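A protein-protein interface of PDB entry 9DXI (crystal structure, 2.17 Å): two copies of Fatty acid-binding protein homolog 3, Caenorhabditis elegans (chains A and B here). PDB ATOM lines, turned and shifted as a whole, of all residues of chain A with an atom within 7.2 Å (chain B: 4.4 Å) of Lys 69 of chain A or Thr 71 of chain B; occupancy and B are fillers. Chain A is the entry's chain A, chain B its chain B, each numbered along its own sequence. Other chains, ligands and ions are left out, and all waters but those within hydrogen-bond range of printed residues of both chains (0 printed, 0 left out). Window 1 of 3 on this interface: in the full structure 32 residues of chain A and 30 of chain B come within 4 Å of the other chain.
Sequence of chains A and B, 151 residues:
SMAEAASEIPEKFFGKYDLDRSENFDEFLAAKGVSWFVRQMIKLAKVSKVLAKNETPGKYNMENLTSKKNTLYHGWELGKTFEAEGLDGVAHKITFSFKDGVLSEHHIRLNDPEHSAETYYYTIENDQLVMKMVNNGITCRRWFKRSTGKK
A ring nitrogen (NE2) of His 74 of chain B lies within hydrogen-bond range of the backbone carbonyl oxygen (O) of Ser 67 of chain A (3.4 Å).
O of Lys 68 of chain A is in hydrogen-bond range of N of His 74 of chain B, at 2.9 Å.
The backbone carbonyl oxygen of Asn 70 of chain A sits at hydrogen-bond distance from the backbone NH of Leu 72 of chain B (2.8 Å).
The backbone NH of Leu 72 of chain A sits at hydrogen-bond distance from the backbone carbonyl oxygen of Asn 70 of chain B (2.7 Å).
N of Asn 64 of chain A lies within hydrogen-bond range of O of Thr 71 of chain A.
O of Lys 69 of chain A is in hydrogen-bond range of OG1 of Thr 66 of chain A (2.9 Å).
The backbone carbonyl oxygen (O) of Met 62 of chain B lies within hydrogen-bond range of the backbone NH (N) of Tyr 73 of chain B.
N of Asn 64 of chain B is in hydrogen-bond range of O of Thr 71 of chain B.
Lys 68 of chain A touches Leu 72 of chain B (O to O, 3.7 Å).
Lys 68 of chain A touches Tyr 73 of chain B.
Lys 69 of chain A touches Tyr 73 of chain B.
CE1 of His 74 of chain B touches N of Lys 69 of chain A, 3.6 Å away.
CB of Lys 69 of chain A touches CB of Ala 84 of chain B (3.7 Å).
CA of Thr 71 of chain B touches O of Asn 70 of chain A (3.5 Å).
His 74 of chain B touches Asn 70 of chain A (CE1 to OD1, 3.2 Å).
Thr 71 of chain A touches Lys 69 of chain B (CG2 to CE, 3.9 Å).
CA of Thr 71 of chain A touches O of Asn 70 of chain B, at 3.4 Å.
Leu 72 of chain A touches Lys 69 of chain B (O to CA, 3.2 Å).
Of the printed residues of chain B, Lys 69 of chain A touches Thr 71 (3.98 Å), Leu 72 (3.3 Å), Tyr 73 (3.5 Å), His 74 (3.6 Å) and Ala 84 (3.7 Å).
Printed residues of chain A within 4 Å of Thr 71 of chain B: Lys 69 (3.98 Å) and Asn 70 (3.5 Å).
Printed residues of chain A within 4 Å of His 74 of chain B: Thr 66 (3.9 Å), Ser 67 (3.4 Å), Lys 68 (2.9 Å), Lys 69 (3.6 Å) and Asn 70 (3.2 Å).
Printed residues of chain A within 4 Å of Lys 69 of chain B: Thr 71 (3.9 Å) and Leu 72 (3.2 Å).
Printed residues of chain B within 4 Å of Thr 71 of chain A: Lys 69 and Asn 70.
Printed residues of chain B within 4 Å of Leu 72 of chain A: Lys 69 (3.2 Å) and Asn 70 (2.7 Å).
The nearest printed residue of chain B that does not touch Lys 69 of chain A is Lys 69 of chain B (6.4 Å).
The nearest printed residue of chain A that does not touch Thr 71 of chain B is Thr 71 of chain A (4.3 Å).
Of the 11 printed residues of chain A, 7 touch a printed residue of chain B.
Hydrophobic or aromatic side chains of chain A that line the printed part of chain B: Leu 72.
Among the printed residues, 18 pairs touch across the chains.
Among the printed residues, no Asp or Glu carboxylate lies within 4 Å of a Lys or Arg side-chain nitrogen of the other chain.
Lys 69 of chain A touches Thr 71 of chain B, and with the chains exchanged Thr 71 of chain A touches Lys 69 of chain B.
Asn 70 of chain B touches its own counterpart, Asn 70 of chain A.
Asn 70 of chain A touches Thr 71 of chain B, and with the chains exchanged Thr 71 of chain A touches Asn 70 of chain B.
Asn 70 of chain A touches Leu 72 of chain B, and with the chains exchanged Leu 72 of chain A touches Asn 70 of chain B.
5 positions are printed for both chains.
Of the 18 pairs that touch across the chains among the printed residues, 9 have their exchanged pair printed and touching as well.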
ATOM      1  N   ASN A  64       5.906 -12.385  17.099  1.00  0.00           N
ATOM      2  CA  ASN A  64       6.378 -11.202  17.802  1.00  0.00           C
ATOM      3  C   ASN A  64       5.158 -10.512  18.394  1.00  0.00           C
ATOM      4  O   ASN A  64       4.242 -10.131  17.656  1.00  0.00           O
ATOM      5  CB  ASN A  64       7.150 -10.272  16.861  1.00  0.00           C
ATOM      6  CG  ASN A  64       7.878  -9.166  17.602  1.00  0.00           C
ATOM      7  OD1 ASN A  64       8.896  -9.406  18.254  1.00  0.00           O
ATOM      8  ND2 ASN A  64       7.364  -7.944  17.500  1.00  0.00           N
ATOM      9  N   LEU A  65       5.131 -10.382  19.717  1.00  0.00           N
ATOM     10  CA  LEU A  65       3.983  -9.853  20.442  1.00  0.00           C
ATOM     11  C   LEU A  65       4.333  -8.515  21.076  1.00  0.00           C
ATOM     12  O   LEU A  65       5.314  -8.411  21.823  1.00  0.00           O
ATOM     13  CB  LEU A  65       3.525 -10.829  21.529  1.00  0.00           C
ATOM     14  CG  LEU A  65       3.325 -12.296  21.158  1.00  0.00           C
ATOM     15  CD1 LEU A  65       3.197 -13.147  22.411  1.00  0.00           C
ATOM     16  CD2 LEU A  65       2.094 -12.450  20.297  1.00  0.00           C
ATOM     17  N   THR A  66       3.528  -7.501  20.789  1.00  0.00           N
ATOM     18  CA  THR A  66       3.606  -6.222  21.474  1.00  0.00           C
ATOM     19  C   THR A  66       2.255  -5.931  22.128  1.00  0.00           C
ATOM     20  O   THR A  66       1.369  -6.791  22.182  1.00  0.00           O
ATOM     21  CB  THR A  66       4.021  -5.101  20.517  1.00  0.00           C
ATOM     22  OG1 THR A  66       2.880  -4.660  19.769  1.00  0.00           O
ATOM     23  CG2 THR A  66       5.098  -5.584  19.559  1.00  0.00           C
ATOM     24  N   SER A  67       2.102  -4.694  22.609  1.00  0.00           N
ATOM     25  CA  SER A  67       0.926  -4.337  23.398  1.00  0.00           C
ATOM     26  C   SER A  67      -0.354  -4.438  22.579  1.00  0.00           C
ATOM     27  O   SER A  67      -1.377  -4.926  23.073  1.00  0.00           O
ATOM     28  CB  SER A  67       1.086  -2.926  23.965  1.00  0.00           C
ATOM     29  OG  SER A  67      -0.126  -2.465  24.532  1.00  0.00           O
ATOM     30  N   LYS A  68      -0.325  -3.975  21.329  1.00  0.00           N
ATOM     31  CA  LYS A  68      -1.509  -4.013  20.486  1.00  0.00           C
ATOM     32  C   LYS A  68      -1.275  -4.604  19.102  1.00  0.00           C
ATOM     33  O   LYS A  68      -2.204  -4.603  18.290  1.00  0.00           O
ATOM     34  CB  LYS A  68      -2.101  -2.602  20.346  1.00  0.00           C
ATOM     35  CG  LYS A  68      -2.893  -2.161  21.566  1.00  0.00           C
ATOM     36  CD  LYS A  68      -3.140  -0.669  21.564  1.00  0.00           C
ATOM     37  CE  LYS A  68      -4.117  -0.272  22.657  1.00  0.00           C
ATOM     38  NZ  LYS A  68      -3.774  -0.900  23.962  1.00  0.00           N
ATOM     39  N   LYS A  69      -0.082  -5.116  18.809  1.00  0.00           N
ATOM     40  CA  LYS A  69       0.208  -5.675  17.495  1.00  0.00           C
ATOM     41  C   LYS A  69       1.000  -6.964  17.643  1.00  0.00           C
ATOM     42  O   LYS A  69       2.029  -6.989  18.325  1.00  0.00           O
ATOM     43  CB  LYS A  69       0.985  -4.680  16.624  1.00  0.00           C
ATOM     44  CG  LYS A  69       1.540  -5.300  15.353  1.00  0.00           C
ATOM     45  CD  LYS A  69       2.292  -4.287  14.506  1.00  0.00           C
ATOM     46  CE  LYS A  69       2.940  -4.967  13.310  1.00  0.00           C
ATOM     47  NZ  LYS A  69       3.440  -3.994  12.300  1.00  0.00           N
ATOM     48  N   ASN A  70       0.516  -8.027  17.003  1.00  0.00           N
ATOM     49  CA  ASN A  70       1.203  -9.309  16.958  1.00  0.00           C
ATOM     50  C   ASN A  70       1.455  -9.697  15.506  1.00  0.00           C
ATOM     51  O   ASN A  70       0.571  -9.556  14.656  1.00  0.00           O
ATOM     52  CB  ASN A  70       0.389 -10.406  17.653  1.00  0.00           C
ATOM     53  CG  ASN A  70       0.056 -10.069  19.097  1.00  0.00           C
ATOM     54  OD1 ASN A  70       0.634  -9.157  19.691  1.00  0.00           O
ATOM     55  ND2 ASN A  70      -0.870 -10.825  19.676  1.00  0.00           N
ATOM     56  N   THR A  71       2.661 -10.184  15.228  1.00  0.00           N
ATOM     57  CA  THR A  71       3.052 -10.617  13.892  1.00  0.00           C
ATOM     58  C   THR A  71       3.481 -12.076  13.952  1.00  0.00           C
ATOM     59  O   THR A  71       4.350 -12.433  14.749  1.00  0.00           O
ATOM     60  CB  THR A  71       4.190  -9.751  13.341  1.00  0.00           C
ATOM     61  OG1 THR A  71       3.799  -8.372  13.363  1.00  0.00           O
ATOM     62  CG2 THR A  71       4.521 -10.153  11.908  1.00  0.00           C
ATOM     63  N   LEU A  72       2.880 -12.910  13.106  1.00  0.00           N
ATOM     64  CA  LEU A  72       3.098 -14.354  13.127  1.00  0.00           C
ATOM     65  C   LEU A  72       3.613 -14.811  11.768  1.00  0.00           C
ATOM     66  O   LEU A  72       2.906 -14.703  10.764  1.00  0.00           O
ATOM     67  CB  LEU A  72       1.805 -15.084  13.488  1.00  0.00           C
ATOM     68  CG  LEU A  72       1.808 -16.605  13.337  1.00  0.00           C
ATOM     69  CD1 LEU A  72       2.766 -17.231  14.329  1.00  0.00           C
ATOM     70  CD2 LEU A  72       0.402 -17.172  13.509  1.00  0.00           C
ATOM     71  N   GLU A  85       3.630 -10.355   2.145  1.00  0.00           N
ATOM     72  CA  GLU A  85       3.022  -9.159   1.517  1.00  0.00           C
ATOM     73  C   GLU A  85       2.174  -8.394   2.531  1.00  0.00           C
ATOM     74  O   GLU A  85       1.229  -8.998   3.074  1.00  0.00           O
ATOM     75  CB  GLU A  85       2.113  -9.616   0.382  1.00  0.00           C
ATOM     76  CG  GLU A  85       2.874 -10.220  -0.794  1.00  0.00           C
ATOM     77  CD  GLU A  85       3.093 -11.716  -0.679  1.00  0.00           C
ATOM     78  OE1 GLU A  85       2.414 -12.342   0.160  1.00  0.00           O
ATOM     79  OE2 GLU A  85       3.942 -12.253  -1.425  1.00  0.00           O
ATOM     80  N   GLY A  86       2.491  -7.116   2.758  1.00  0.00           N
ATOM     81  CA  GLY A  86       1.728  -6.289   3.713  1.00  0.00           C
ATOM     82  C   GLY A  86       0.768  -5.357   2.998  1.00  0.00           C
ATOM     83  O   GLY A  86       0.926  -5.177   1.772  1.00  0.00           O
ATOM     84  N   MET B  62      -8.377  -6.281  14.432  1.00  0.00           N
ATOM     85  CA  MET B  62      -8.289  -6.439  12.990  1.00  0.00           C
ATOM     86  C   MET B  62      -7.104  -7.333  12.665  1.00  0.00           C
ATOM     87  O   MET B  62      -6.009  -7.131  13.198  1.00  0.00           O
ATOM     88  CB  MET B  62      -8.140  -5.108  12.261  1.00  0.00           C
ATOM     89  CG  MET B  62      -7.986  -5.327  10.761  1.00  0.00           C
ATOM     90  SD  MET B  62      -8.505  -3.971   9.712  1.00  0.00           S
ATOM     91  CE  MET B  62      -6.930  -3.199   9.410  1.00  0.00           C
ATOM     92  N   GLU B  63      -7.321  -8.308  11.784  1.00  0.00           N
ATOM     93  CA  GLU B  63      -6.304  -9.279  11.417  1.00  0.00           C
ATOM     94  C   GLU B  63      -6.105  -9.292   9.909  1.00  0.00           C
ATOM     95  O   GLU B  63      -7.063  -9.149   9.145  1.00  0.00           O
ATOM     96  CB  GLU B  63      -6.676 -10.684  11.913  1.00  0.00           C
ATOM     97  CG  GLU B  63      -5.543 -11.690  11.799  1.00  0.00           C
ATOM     98  CD  GLU B  63      -5.719 -12.892  12.712  1.00  0.00           C
ATOM     99  OE1 GLU B  63      -6.867 -13.190  13.096  1.00  0.00           O
ATOM    100  OE2 GLU B  63      -4.698 -13.535  13.049  1.00  0.00           O
ATOM    101  N   ASN B  64      -4.849  -9.470   9.505  1.00  0.00           N
ATOM    102  CA  ASN B  64      -4.491  -9.648   8.078  1.00  0.00           C
ATOM    103  C   ASN B  64      -3.884 -11.050   7.964  1.00  0.00           C
ATOM    104  O   ASN B  64      -2.898 -11.302   8.660  1.00  0.00           O
ATOM    105  CB  ASN B  64      -3.573  -8.539   7.596  1.00  0.00           C
ATOM    106  CG  ASN B  64      -4.316  -7.495   6.805  1.00  0.00           C
ATOM    107  OD1 ASN B  64      -4.703  -6.461   7.355  1.00  0.00           O
ATOM    108  ND2 ASN B  64      -4.523  -7.750   5.522  1.00  0.00           N
ATOM    109  N   LYS B  69       2.398 -15.046   6.687  1.00  0.00           N
ATOM    110  CA  LYS B  69       2.510 -13.954   7.648  1.00  0.00           C
ATOM    111  C   LYS B  69       1.120 -13.479   8.045  1.00  0.00           C
ATOM    112  O   LYS B  69       0.344 -13.047   7.190  1.00  0.00           O
ATOM    113  CB  LYS B  69       3.318 -12.794   7.060  1.00  0.00           C
ATOM    114  CG  LYS B  69       3.424 -11.587   7.983  1.00  0.00           C
ATOM    115  CD  LYS B  69       4.155 -10.433   7.310  1.00  0.00           C
ATOM    116  CE  LYS B  69       4.108  -9.173   8.163  1.00  0.00           C
ATOM    117  NZ  LYS B  69       4.756  -8.016   7.486  1.00  0.00           N
ATOM    118  N   ASN B  70       0.806 -13.556   9.334  1.00  0.00           N
ATOM    119  CA  ASN B  70      -0.411 -12.977   9.884  1.00  0.00           C
ATOM    120  C   ASN B  70      -0.050 -11.785  10.756  1.00  0.00           C
ATOM    121  O   ASN B  70       0.896 -11.855  11.547  1.00  0.00           O
ATOM    122  CB  ASN B  70      -1.198 -14.004  10.699  1.00  0.00           C
ATOM    123  CG  ASN B  70      -1.669 -15.161   9.860  1.00  0.00           C
ATOM    124  OD1 ASN B  70      -1.688 -15.078   8.632  1.00  0.00           O
ATOM    125  ND2 ASN B  70      -2.062 -16.248  10.514  1.00  0.00           N
ATOM    126  N   THR B  71      -0.800 -10.699  10.608  1.00  0.00           N
ATOM    127  CA  THR B  71      -0.643  -9.503  11.422  1.00  0.00           C
ATOM    128  C   THR B  71      -1.958  -9.237  12.139  1.00  0.00           C
ATOM    129  O   THR B  71      -3.025  -9.292  11.523  1.00  0.00           O
ATOM    130  CB  THR B  71      -0.243  -8.299  10.565  1.00  0.00           C
ATOM    131  OG1 THR B  71       0.869  -8.659   9.737  1.00  0.00           O
ATOM    132  CG2 THR B  71       0.155  -7.124  11.448  1.00  0.00           C
ATOM    133  N   LEU B  72      -1.882  -8.956  13.436  1.00  0.00           N
ATOM    134  CA  LEU B  72      -3.068  -8.853  14.280  1.00  0.00           C
ATOM    135  C   LEU B  72      -2.960  -7.597  15.137  1.00  0.00           C
ATOM    136  O   LEU B  72      -2.077  -7.501  15.993  1.00  0.00           O
ATOM    137  CB  LEU B  72      -3.219 -10.109  15.136  1.00  0.00           C
ATOM    138  CG  LEU B  72      -4.420 -10.271  16.071  1.00  0.00           C
ATOM    139  CD1 LEU B  72      -4.096  -9.722  17.444  1.00  0.00           C
ATOM    140  CD2 LEU B  72      -5.672  -9.614  15.503  1.00  0.00           C
ATOM    141  N   TYR B  73      -3.851  -6.633  14.898  1.00  0.00           N
ATOM    142  CA  TYR B  73      -3.986  -5.448  15.742  1.00  0.00           C
ATOM    143  C   TYR B  73      -5.160  -5.682  16.686  1.00  0.00           C
ATOM    144  O   TYR B  73      -6.310  -5.769  16.244  1.00  0.00           O
ATOM    145  CB  TYR B  73      -4.205  -4.193  14.901  1.00  0.00           C
ATOM    146  CG  TYR B  73      -3.087  -3.874  13.932  1.00  0.00           C
ATOM    147  CD1 TYR B  73      -1.878  -3.355  14.378  1.00  0.00           C
ATOM    148  CD2 TYR B  73      -3.250  -4.074  12.566  1.00  0.00           C
ATOM    149  CE1 TYR B  73      -0.858  -3.056  13.492  1.00  0.00           C
ATOM    150  CE2 TYR B  73      -2.234  -3.778  11.674  1.00  0.00           C
ATOM    151  CZ  TYR B  73      -1.041  -3.269  12.141  1.00  0.00           C
ATOM    152  OH  TYR B  73      -0.030  -2.974  11.254  1.00  0.00           O
ATOM    153  N   HIS B  74      -4.878  -5.777  17.984  1.00  0.00           N
ATOM    154  CA  HIS B  74      -5.883  -6.145  18.969  1.00  0.00           C
ATOM    155  C   HIS B  74      -5.987  -5.104  20.076  1.00  0.00           C
ATOM    156  O   HIS B  74      -5.017  -4.411  20.401  1.00  0.00           O
ATOM    157  CB  HIS B  74      -5.583  -7.512  19.590  1.00  0.00           C
ATOM    158  CG  HIS B  74      -4.255  -7.591  20.280  1.00  0.00           C
ATOM    159  ND1 HIS B  74      -3.058  -7.434  19.613  1.00  0.00           N
ATOM    160  CD2 HIS B  74      -3.936  -7.827  21.573  1.00  0.00           C
ATOM    161  CE1 HIS B  74      -2.060  -7.564  20.468  1.00  0.00           C
ATOM    162  NE2 HIS B  74      -2.565  -7.803  21.664  1.00  0.00           N
ATOM    163  N   ALA B  84       3.275   0.723  18.145  1.00  0.00           N
ATOM    164  CA  ALA B  84       3.742  -0.650  18.060  1.00  0.00           C
ATOM    165  C   ALA B  84       5.152  -0.652  17.496  1.00  0.00           C
ATOM    166  O   ALA B  84       5.484   0.164  16.632  1.00  0.00           O
ATOM    167  CB  ALA B  84       2.820  -1.509  17.188  1.00  0.00           C
